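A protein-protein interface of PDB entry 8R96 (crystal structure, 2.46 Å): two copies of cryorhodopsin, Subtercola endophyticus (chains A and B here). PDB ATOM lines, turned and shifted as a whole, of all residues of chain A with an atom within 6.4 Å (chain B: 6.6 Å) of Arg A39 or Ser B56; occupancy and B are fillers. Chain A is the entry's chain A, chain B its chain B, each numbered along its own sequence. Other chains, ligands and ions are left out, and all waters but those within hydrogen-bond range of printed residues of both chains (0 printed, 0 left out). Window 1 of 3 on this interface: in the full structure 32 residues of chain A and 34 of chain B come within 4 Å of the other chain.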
ATOM      1  N   VAL A  34       5.650  -0.154   1.491  1.00  0.00           N
ATOM      2  CA  VAL A  34       5.199   1.159   2.043  1.00  0.00           C
ATOM      3  C   VAL A  34       5.911   1.386   3.380  1.00  0.00           C
ATOM      4  O   VAL A  34       6.565   2.434   3.532  1.00  0.00           O
ATOM      5  CB  VAL A  34       3.667   1.214   2.208  1.00  0.00           C
ATOM      6  CG1 VAL A  34       3.239   2.293   3.190  1.00  0.00           C
ATOM      7  CG2 VAL A  34       2.963   1.391   0.872  1.00  0.00           C
ATOM      8  N   ALA A  35       5.784   0.430   4.307  1.00  0.00           N
ATOM      9  CA  ALA A  35       6.401   0.453   5.653  1.00  0.00           C
ATOM     10  C   ALA A  35       7.919   0.617   5.517  1.00  0.00           C
ATOM     11  O   ALA A  35       8.496   1.438   6.258  1.00  0.00           O
ATOM     12  CB  ALA A  35       6.050  -0.809   6.402  1.00  0.00           C
ATOM     13  N   GLY A  36       8.531  -0.146   4.605  1.00  0.00           N
ATOM     14  CA  GLY A  36       9.976  -0.098   4.315  1.00  0.00           C
ATOM     15  C   GLY A  36      10.389   1.275   3.818  1.00  0.00           C
ATOM     16  O   GLY A  36      11.341   1.852   4.385  1.00  0.00           O
ATOM     17  N   PHE A  37       9.685   1.783   2.802  1.00  0.00           N
ATOM     18  CA  PHE A  37       9.924   3.112   2.183  1.00  0.00           C
ATOM     19  C   PHE A  37       9.924   4.182   3.277  1.00  0.00           C
ATOM     20  O   PHE A  37      10.878   4.977   3.344  1.00  0.00           O
ATOM     21  CB  PHE A  37       8.866   3.425   1.123  1.00  0.00           C
ATOM     22  CG  PHE A  37       9.105   4.723   0.397  1.00  0.00           C
ATOM     23  CD1 PHE A  37       9.808   4.747  -0.797  1.00  0.00           C
ATOM     24  CD2 PHE A  37       8.658   5.923   0.926  1.00  0.00           C
ATOM     25  CE1 PHE A  37      10.042   5.944  -1.454  1.00  0.00           C
ATOM     26  CE2 PHE A  37       8.893   7.118   0.268  1.00  0.00           C
ATOM     27  CZ  PHE A  37       9.585   7.126  -0.921  1.00  0.00           C
ATOM     28  N   ILE A  38       8.879   4.195   4.107  1.00  0.00           N
ATOM     29  CA  ILE A  38       8.697   5.171   5.221  1.00  0.00           C
ATOM     30  C   ILE A  38       9.899   5.067   6.166  1.00  0.00           C
ATOM     31  O   ILE A  38      10.554   6.101   6.401  1.00  0.00           O
ATOM     32  CB  ILE A  38       7.363   4.928   5.952  1.00  0.00           C
ATOM     33  CG1 ILE A  38       6.166   5.195   5.037  1.00  0.00           C
ATOM     34  CG2 ILE A  38       7.289   5.754   7.225  1.00  0.00           C
ATOM     35  CD1 ILE A  38       4.826   4.958   5.693  1.00  0.00           C
ATOM     36  N   ARG A  39      10.179   3.868   6.683  1.00  0.00           N
ATOM     37  CA  ARG A  39      11.318   3.627   7.608  1.00  0.00           C
ATOM     38  C   ARG A  39      12.594   4.192   6.978  1.00  0.00           C
ATOM     39  O   ARG A  39      13.288   4.977   7.651  1.00  0.00           O
ATOM     40  CB  ARG A  39      11.498   2.137   7.912  1.00  0.00           C
ATOM     41  CG  ARG A  39      12.633   1.853   8.886  1.00  0.00           C
ATOM     42  CD  ARG A  39      12.903   0.369   9.057  1.00  0.00           C
ATOM     43  NE  ARG A  39      13.007  -0.024  10.457  1.00  0.00           N
ATOM     44  CZ  ARG A  39      13.306  -1.247  10.880  1.00  0.00           C
ATOM     45  NH1 ARG A  39      13.545  -2.214  10.011  1.00  0.00           N
ATOM     46  NH2 ARG A  39      13.368  -1.501  12.176  1.00  0.00           N
ATOM     47  N   THR A  40      12.875   3.810   5.729  1.00  0.00           N
ATOM     48  CA  THR A  40      14.103   4.197   4.985  1.00  0.00           C
ATOM     49  C   THR A  40      14.209   5.724   4.920  1.00  0.00           C
ATOM     50  O   THR A  40      15.318   6.250   5.162  1.00  0.00           O
ATOM     51  CB  THR A  40      14.122   3.584   3.580  1.00  0.00           C
ATOM     52  OG1 THR A  40      14.292   2.173   3.719  1.00  0.00           O
ATOM     53  CG2 THR A  40      15.224   4.151   2.711  1.00  0.00           C
ATOM     54  N   TYR A  41      13.104   6.403   4.601  1.00  0.00           N
ATOM     55  CA  TYR A  41      13.033   7.880   4.460  1.00  0.00           C
ATOM     56  C   TYR A  41      13.366   8.537   5.805  1.00  0.00           C
ATOM     57  O   TYR A  41      14.185   9.466   5.832  1.00  0.00           O
ATOM     58  CB  TYR A  41      11.657   8.323   3.956  1.00  0.00           C
ATOM     59  CG  TYR A  41      11.522   9.815   3.786  1.00  0.00           C
ATOM     60  CD1 TYR A  41      10.866  10.586   4.731  1.00  0.00           C
ATOM     61  CD2 TYR A  41      12.080  10.464   2.697  1.00  0.00           C
ATOM     62  CE1 TYR A  41      10.749  11.959   4.590  1.00  0.00           C
ATOM     63  CE2 TYR A  41      11.978  11.836   2.543  1.00  0.00           C
ATOM     64  CZ  TYR A  41      11.308  12.588   3.491  1.00  0.00           C
ATOM     65  OH  TYR A  41      11.202  13.941   3.344  1.00  0.00           O
ATOM     66  N   ILE A  42      12.749   8.062   6.888  1.00  0.00           N
ATOM     67  CA  ILE A  42      12.853   8.666   8.251  1.00  0.00           C
ATOM     68  C   ILE A  42      14.285   8.509   8.777  1.00  0.00           C
ATOM     69  O   ILE A  42      14.747   9.415   9.497  1.00  0.00           O
ATOM     70  CB  ILE A  42      11.811   8.042   9.200  1.00  0.00           C
ATOM     71  CG1 ILE A  42      10.420   8.631   8.953  1.00  0.00           C
ATOM     72  CG2 ILE A  42      12.234   8.180  10.655  1.00  0.00           C
ATOM     73  CD1 ILE A  42       9.614   8.854  10.214  1.00  0.00           C
ATOM     74  N   THR A  43      14.958   7.408   8.427  1.00  0.00           N
ATOM     75  CA  THR A  43      16.307   7.042   8.935  1.00  0.00           C
ATOM     76  C   THR A  43      17.385   7.433   7.917  1.00  0.00           C
ATOM     77  O   THR A  43      18.494   6.869   7.989  1.00  0.00           O
ATOM     78  CB  THR A  43      16.377   5.545   9.264  1.00  0.00           C
ATOM     79  OG1 THR A  43      16.176   4.806   8.058  1.00  0.00           O
ATOM     80  CG2 THR A  43      15.353   5.127  10.297  1.00  0.00           C
ATOM     81  N   ARG A  44      17.083   8.377   7.020  1.00  0.00           N
ATOM     82  CA  ARG A  44      17.973   8.756   5.889  1.00  0.00           C
ATOM     83  C   ARG A  44      19.194   9.521   6.420  1.00  0.00           C
ATOM     84  O   ARG A  44      20.296   9.327   5.868  1.00  0.00           O
ATOM     85  CB  ARG A  44      17.201   9.572   4.845  1.00  0.00           C
ATOM     86  CG  ARG A  44      16.793  10.970   5.290  1.00  0.00           C
ATOM     87  CD  ARG A  44      15.896  11.649   4.267  1.00  0.00           C
ATOM     88  NE  ARG A  44      15.596  13.035   4.599  1.00  0.00           N
ATOM     89  CZ  ARG A  44      14.568  13.431   5.342  1.00  0.00           C
ATOM     90  NH1 ARG A  44      13.724  12.544   5.839  1.00  0.00           N
ATOM     91  NH2 ARG A  44      14.381  14.717   5.584  1.00  0.00           N
ATOM     92  N   LEU A  59      15.898   3.775  -1.137  1.00  0.00           N
ATOM     93  CA  LEU A  59      14.589   4.474  -1.192  1.00  0.00           C
ATOM     94  C   LEU A  59      14.053   4.409  -2.626  1.00  0.00           C
ATOM     95  O   LEU A  59      12.847   4.137  -2.797  1.00  0.00           O
ATOM     96  CB  LEU A  59      14.763   5.919  -0.721  1.00  0.00           C
ATOM     97  CG  LEU A  59      13.486   6.591  -0.217  1.00  0.00           C
ATOM     98  CD1 LEU A  59      12.837   5.767   0.883  1.00  0.00           C
ATOM     99  CD2 LEU A  59      13.768   8.000   0.275  1.00  0.00           C
ATOM    100  N   THR A 247      18.172  -3.536   4.779  1.00  0.00           N
ATOM    101  CA  THR A 247      18.449  -3.355   6.229  1.00  0.00           C
ATOM    102  C   THR A 247      19.952  -3.510   6.483  1.00  0.00           C
ATOM    103  O   THR A 247      20.485  -2.757   7.318  1.00  0.00           O
ATOM    104  CB  THR A 247      17.656  -4.345   7.092  1.00  0.00           C
ATOM    105  OG1 THR A 247      16.277  -4.265   6.729  1.00  0.00           O
ATOM    106  CG2 THR A 247      17.820  -4.073   8.572  1.00  0.00           C
ATOM    107  N   THR B  40       2.092  11.935  14.064  1.00  0.00           N
ATOM    108  CA  THR B  40       3.305  11.094  14.254  1.00  0.00           C
ATOM    109  C   THR B  40       4.477  11.688  13.468  1.00  0.00           C
ATOM    110  O   THR B  40       5.577  11.790  14.046  1.00  0.00           O
ATOM    111  CB  THR B  40       3.050   9.643  13.838  1.00  0.00           C
ATOM    112  OG1 THR B  40       2.131   9.088  14.780  1.00  0.00           O
ATOM    113  CG2 THR B  40       4.318   8.818  13.785  1.00  0.00           C
ATOM    114  N   TYR B  51      15.955   6.040  19.772  1.00  0.00           N
ATOM    115  CA  TYR B  51      14.576   5.498  19.885  1.00  0.00           C
ATOM    116  C   TYR B  51      13.792   5.785  18.598  1.00  0.00           C
ATOM    117  O   TYR B  51      12.548   5.787  18.644  1.00  0.00           O
ATOM    118  CB  TYR B  51      13.879   6.092  21.111  1.00  0.00           C
ATOM    119  CG  TYR B  51      14.631   5.903  22.403  1.00  0.00           C
ATOM    120  CD1 TYR B  51      14.703   4.659  23.008  1.00  0.00           C
ATOM    121  CD2 TYR B  51      15.275   6.962  23.021  1.00  0.00           C
ATOM    122  CE1 TYR B  51      15.390   4.471  24.195  1.00  0.00           C
ATOM    123  CE2 TYR B  51      15.969   6.791  24.208  1.00  0.00           C
ATOM    124  CZ  TYR B  51      16.028   5.540  24.797  1.00  0.00           C
ATOM    125  OH  TYR B  51      16.710   5.355  25.963  1.00  0.00           O
ATOM    126  N   ARG B  52      14.497   5.997  17.483  1.00  0.00           N
ATOM    127  CA  ARG B  52      13.886   6.361  16.177  1.00  0.00           C
ATOM    128  C   ARG B  52      13.112   5.167  15.608  1.00  0.00           C
ATOM    129  O   ARG B  52      12.108   5.401  14.907  1.00  0.00           O
ATOM    130  CB  ARG B  52      14.951   6.829  15.182  1.00  0.00           C
ATOM    131  CG  ARG B  52      14.375   7.344  13.871  1.00  0.00           C
ATOM    132  CD  ARG B  52      15.345   8.266  13.161  1.00  0.00           C
ATOM    133  NE  ARG B  52      15.727   9.396  13.997  1.00  0.00           N
ATOM    134  CZ  ARG B  52      16.898  10.018  13.931  1.00  0.00           C
ATOM    135  NH1 ARG B  52      17.818   9.612  13.070  1.00  0.00           N
ATOM    136  NH2 ARG B  52      17.152  11.035  14.734  1.00  0.00           N
ATOM    137  N   THR B  53      13.564   3.941  15.891  1.00  0.00           N
ATOM    138  CA  THR B  53      12.922   2.684  15.424  1.00  0.00           C
ATOM    139  C   THR B  53      11.465   2.668  15.896  1.00  0.00           C
ATOM    140  O   THR B  53      10.615   2.116  15.169  1.00  0.00           O
ATOM    141  CB  THR B  53      13.675   1.442  15.916  1.00  0.00           C
ATOM    142  OG1 THR B  53      15.069   1.640  15.677  1.00  0.00           O
ATOM    143  CG2 THR B  53      13.214   0.171  15.235  1.00  0.00           C
ATOM    144  N   ALA B  54      11.197   3.254  17.068  1.00  0.00           N
ATOM    145  CA  ALA B  54       9.848   3.390  17.663  1.00  0.00           C
ATOM    146  C   ALA B  54       8.977   4.247  16.742  1.00  0.00           C
ATOM    147  O   ALA B  54       7.793   3.903  16.555  1.00  0.00           O
ATOM    148  CB  ALA B  54       9.944   3.995  19.041  1.00  0.00           C
ATOM    149  N   VAL B  55       9.559   5.314  16.187  1.00  0.00           N
ATOM    150  CA  VAL B  55       8.857   6.326  15.343  1.00  0.00           C
ATOM    151  C   VAL B  55       8.590   5.724  13.960  1.00  0.00           C
ATOM    152  O   VAL B  55       7.424   5.754  13.526  1.00  0.00           O
ATOM    153  CB  VAL B  55       9.670   7.630  15.240  1.00  0.00           C
ATOM    154  CG1 VAL B  55       8.994   8.651  14.337  1.00  0.00           C
ATOM    155  CG2 VAL B  55       9.938   8.230  16.611  1.00  0.00           C
ATOM    156  N   SER B  56       9.628   5.206  13.298  1.00  0.00           N
ATOM    157  CA  SER B  56       9.548   4.616  11.934  1.00  0.00           C
ATOM    158  C   SER B  56       8.501   3.497  11.918  1.00  0.00           C
ATOM    159  O   SER B  56       7.760   3.396  10.920  1.00  0.00           O
ATOM    160  CB  SER B  56      10.894   4.122  11.463  1.00  0.00           C
ATOM    161  OG  SER B  56      11.430   3.161  12.361  1.00  0.00           O
ATOM    162  N   ALA B  57       8.443   2.695  12.985  1.00  0.00           N
ATOM    163  CA  ALA B  57       7.471   1.591  13.160  1.00  0.00           C
ATOM    164  C   ALA B  57       6.058   2.173  13.278  1.00  0.00           C
ATOM    165  O   ALA B  57       5.163   1.707  12.543  1.00  0.00           O
ATOM    166  CB  ALA B  57       7.836   0.768  14.370  1.00  0.00           C
ATOM    167  N   ARG B  58       5.871   3.157  14.164  1.00  0.00           N
ATOM    168  CA  ARG B  58       4.559   3.807  14.425  1.00  0.00           C
ATOM    169  C   ARG B  58       4.033   4.409  13.115  1.00  0.00           C
ATOM    170  O   ARG B  58       2.873   4.132  12.761  1.00  0.00           O
ATOM    171  CB  ARG B  58       4.682   4.870  15.522  1.00  0.00           C
ATOM    172  CG  ARG B  58       3.368   5.556  15.869  1.00  0.00           C
ATOM    173  CD  ARG B  58       3.373   6.261  17.217  1.00  0.00           C
ATOM    174  NE  ARG B  58       4.528   7.132  17.418  1.00  0.00           N
ATOM    175  CZ  ARG B  58       5.594   6.822  18.153  1.00  0.00           C
ATOM    176  NH1 ARG B  58       5.664   5.650  18.761  1.00  0.00           N
ATOM    177  NH2 ARG B  58       6.588   7.684  18.276  1.00  0.00           N
ATOM    178  N   LEU B  59       4.863   5.193  12.422  1.00  0.00           N
ATOM    179  CA  LEU B  59       4.494   5.862  11.146  1.00  0.00           C
ATOM    180  C   LEU B  59       4.227   4.792  10.085  1.00  0.00           C
ATOM    181  O   LEU B  59       3.222   4.912   9.365  1.00  0.00           O
ATOM    182  CB  LEU B  59       5.624   6.802  10.718  1.00  0.00           C
ATOM    183  CG  LEU B  59       5.205   7.924   9.771  1.00  0.00           C
ATOM    184  CD1 LEU B  59       4.079   8.751  10.376  1.00  0.00           C
ATOM    185  CD2 LEU B  59       6.391   8.807   9.421  1.00  0.00           C
ATOM    186  N   GLY B  60       5.099   3.784  10.006  1.00  0.00           N
ATOM    187  CA  GLY B  60       4.940   2.627   9.108  1.00  0.00           C
ATOM    188  C   GLY B  60       3.580   1.972   9.286  1.00  0.00           C
ATOM    189  O   GLY B  60       2.896   1.748   8.267  1.00  0.00           O
ATOM    190  N   MET B  61       3.191   1.689  10.535  1.00  0.00           N
ATOM    191  CA  MET B  61       1.944   0.946  10.862  1.00  0.00           C
ATOM    192  C   MET B  61       0.726   1.820  10.538  1.00  0.00           C
ATOM    193  O   MET B  61      -0.257   1.274   9.995  1.00  0.00           O
ATOM    194  CB  MET B  61       1.898   0.533  12.337  1.00  0.00           C
ATOM    195  CG  MET B  61       1.601   1.682  13.282  1.00  0.00           C
ATOM    196  SD  MET B  61       0.252   1.311  14.429  1.00  0.00           S
ATOM    197  CE  MET B  61      -0.867   0.442  13.331  1.00  0.00           C
ATOM    198  N   LEU B 110       4.546  -4.714  13.119  1.00  0.00           N
ATOM    199  CA  LEU B 110       5.096  -3.345  13.316  1.00  0.00           C
ATOM    200  C   LEU B 110       4.827  -2.897  14.756  1.00  0.00           C
ATOM    201  O   LEU B 110       5.689  -2.205  15.329  1.00  0.00           O
ATOM    202  CB  LEU B 110       4.456  -2.388  12.307  1.00  0.00           C
ATOM    203  CG  LEU B 110       4.945  -2.542  10.867  1.00  0.00           C
ATOM    204  CD1 LEU B 110       4.180  -1.617   9.935  1.00  0.00           C
ATOM    205  CD2 LEU B 110       6.441  -2.285  10.769  1.00  0.00           C
ATOM    206  N   ILE B 113       7.521  -4.584  17.006  1.00  0.00           N
ATOM    207  CA  ILE B 113       8.793  -3.837  16.772  1.00  0.00           C
ATOM    208  C   ILE B 113       8.759  -2.528  17.569  1.00  0.00           C
ATOM    209  O   ILE B 113       9.773  -2.203  18.223  1.00  0.00           O
ATOM    210  CB  ILE B 113       8.997  -3.578  15.265  1.00  0.00           C
ATOM    211  CG1 ILE B 113       9.190  -4.882  14.489  1.00  0.00           C
ATOM    212  CG2 ILE B 113      10.147  -2.609  15.035  1.00  0.00           C
ATOM    213  CD1 ILE B 113       8.922  -4.761  13.009  1.00  0.00           C
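The backbone carbonyl oxygen (O) of Arg B52 sits at hydrogen-bond distance from the side-chain hydroxyl (OG) of Ser B56 (3.5 Å).
O of Thr B53 lies within hydrogen-bond range of OG of Ser B56 (3.1 Å).
O of Arg A39 lies within hydrogen-bond range of OG1 of Thr A43, at 2.9 Å.
Ile A38 touches Leu B59 (CG2 to CD2, 3.9 Å).
Arg A39 touches Thr B53.
CG of Arg A39 touches CB of Ser B56, at 3.8 Å.
Arg B52 touches Ile A42.
Leu B59 touches Ile A42 (CD2 to CD1, 3.3 Å).
Phe A37 touches none of the printed residues of chain B.
Of the printed residues of chain B, Ile A38 touches Leu B59.
Of chain B, only Thr B53 (3.5 Å) and Ser B56 (3.8 Å) come within 4 Å of Arg A39.
Of the printed residues of chain B, Ile A42 touches Arg B52 and Leu B59.
Of the printed residues of chain A, Arg B52 touches Ile A42.
Of the printed residues of chain A, Thr B53 touches Arg A39 (3.5 Å).
Leu B110 touches none of the printed residues of chain A.
The nearest residue of chain A that does not touch Ser B56 is Ile A42 (4.3 Å).
Hydrophobic or aromatic side chains of chain B that line the printed part of chain A: Leu B59.
Hydrophobic or aromatic side chains of chain A within 4 Å of the printed part of chain B: Ile A38 and Ile A42.
2 positions are printed for both chains.
Of the 5 pairs that touch across the chains among the printed residues, none has its exchanged pair printed and touching as well.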
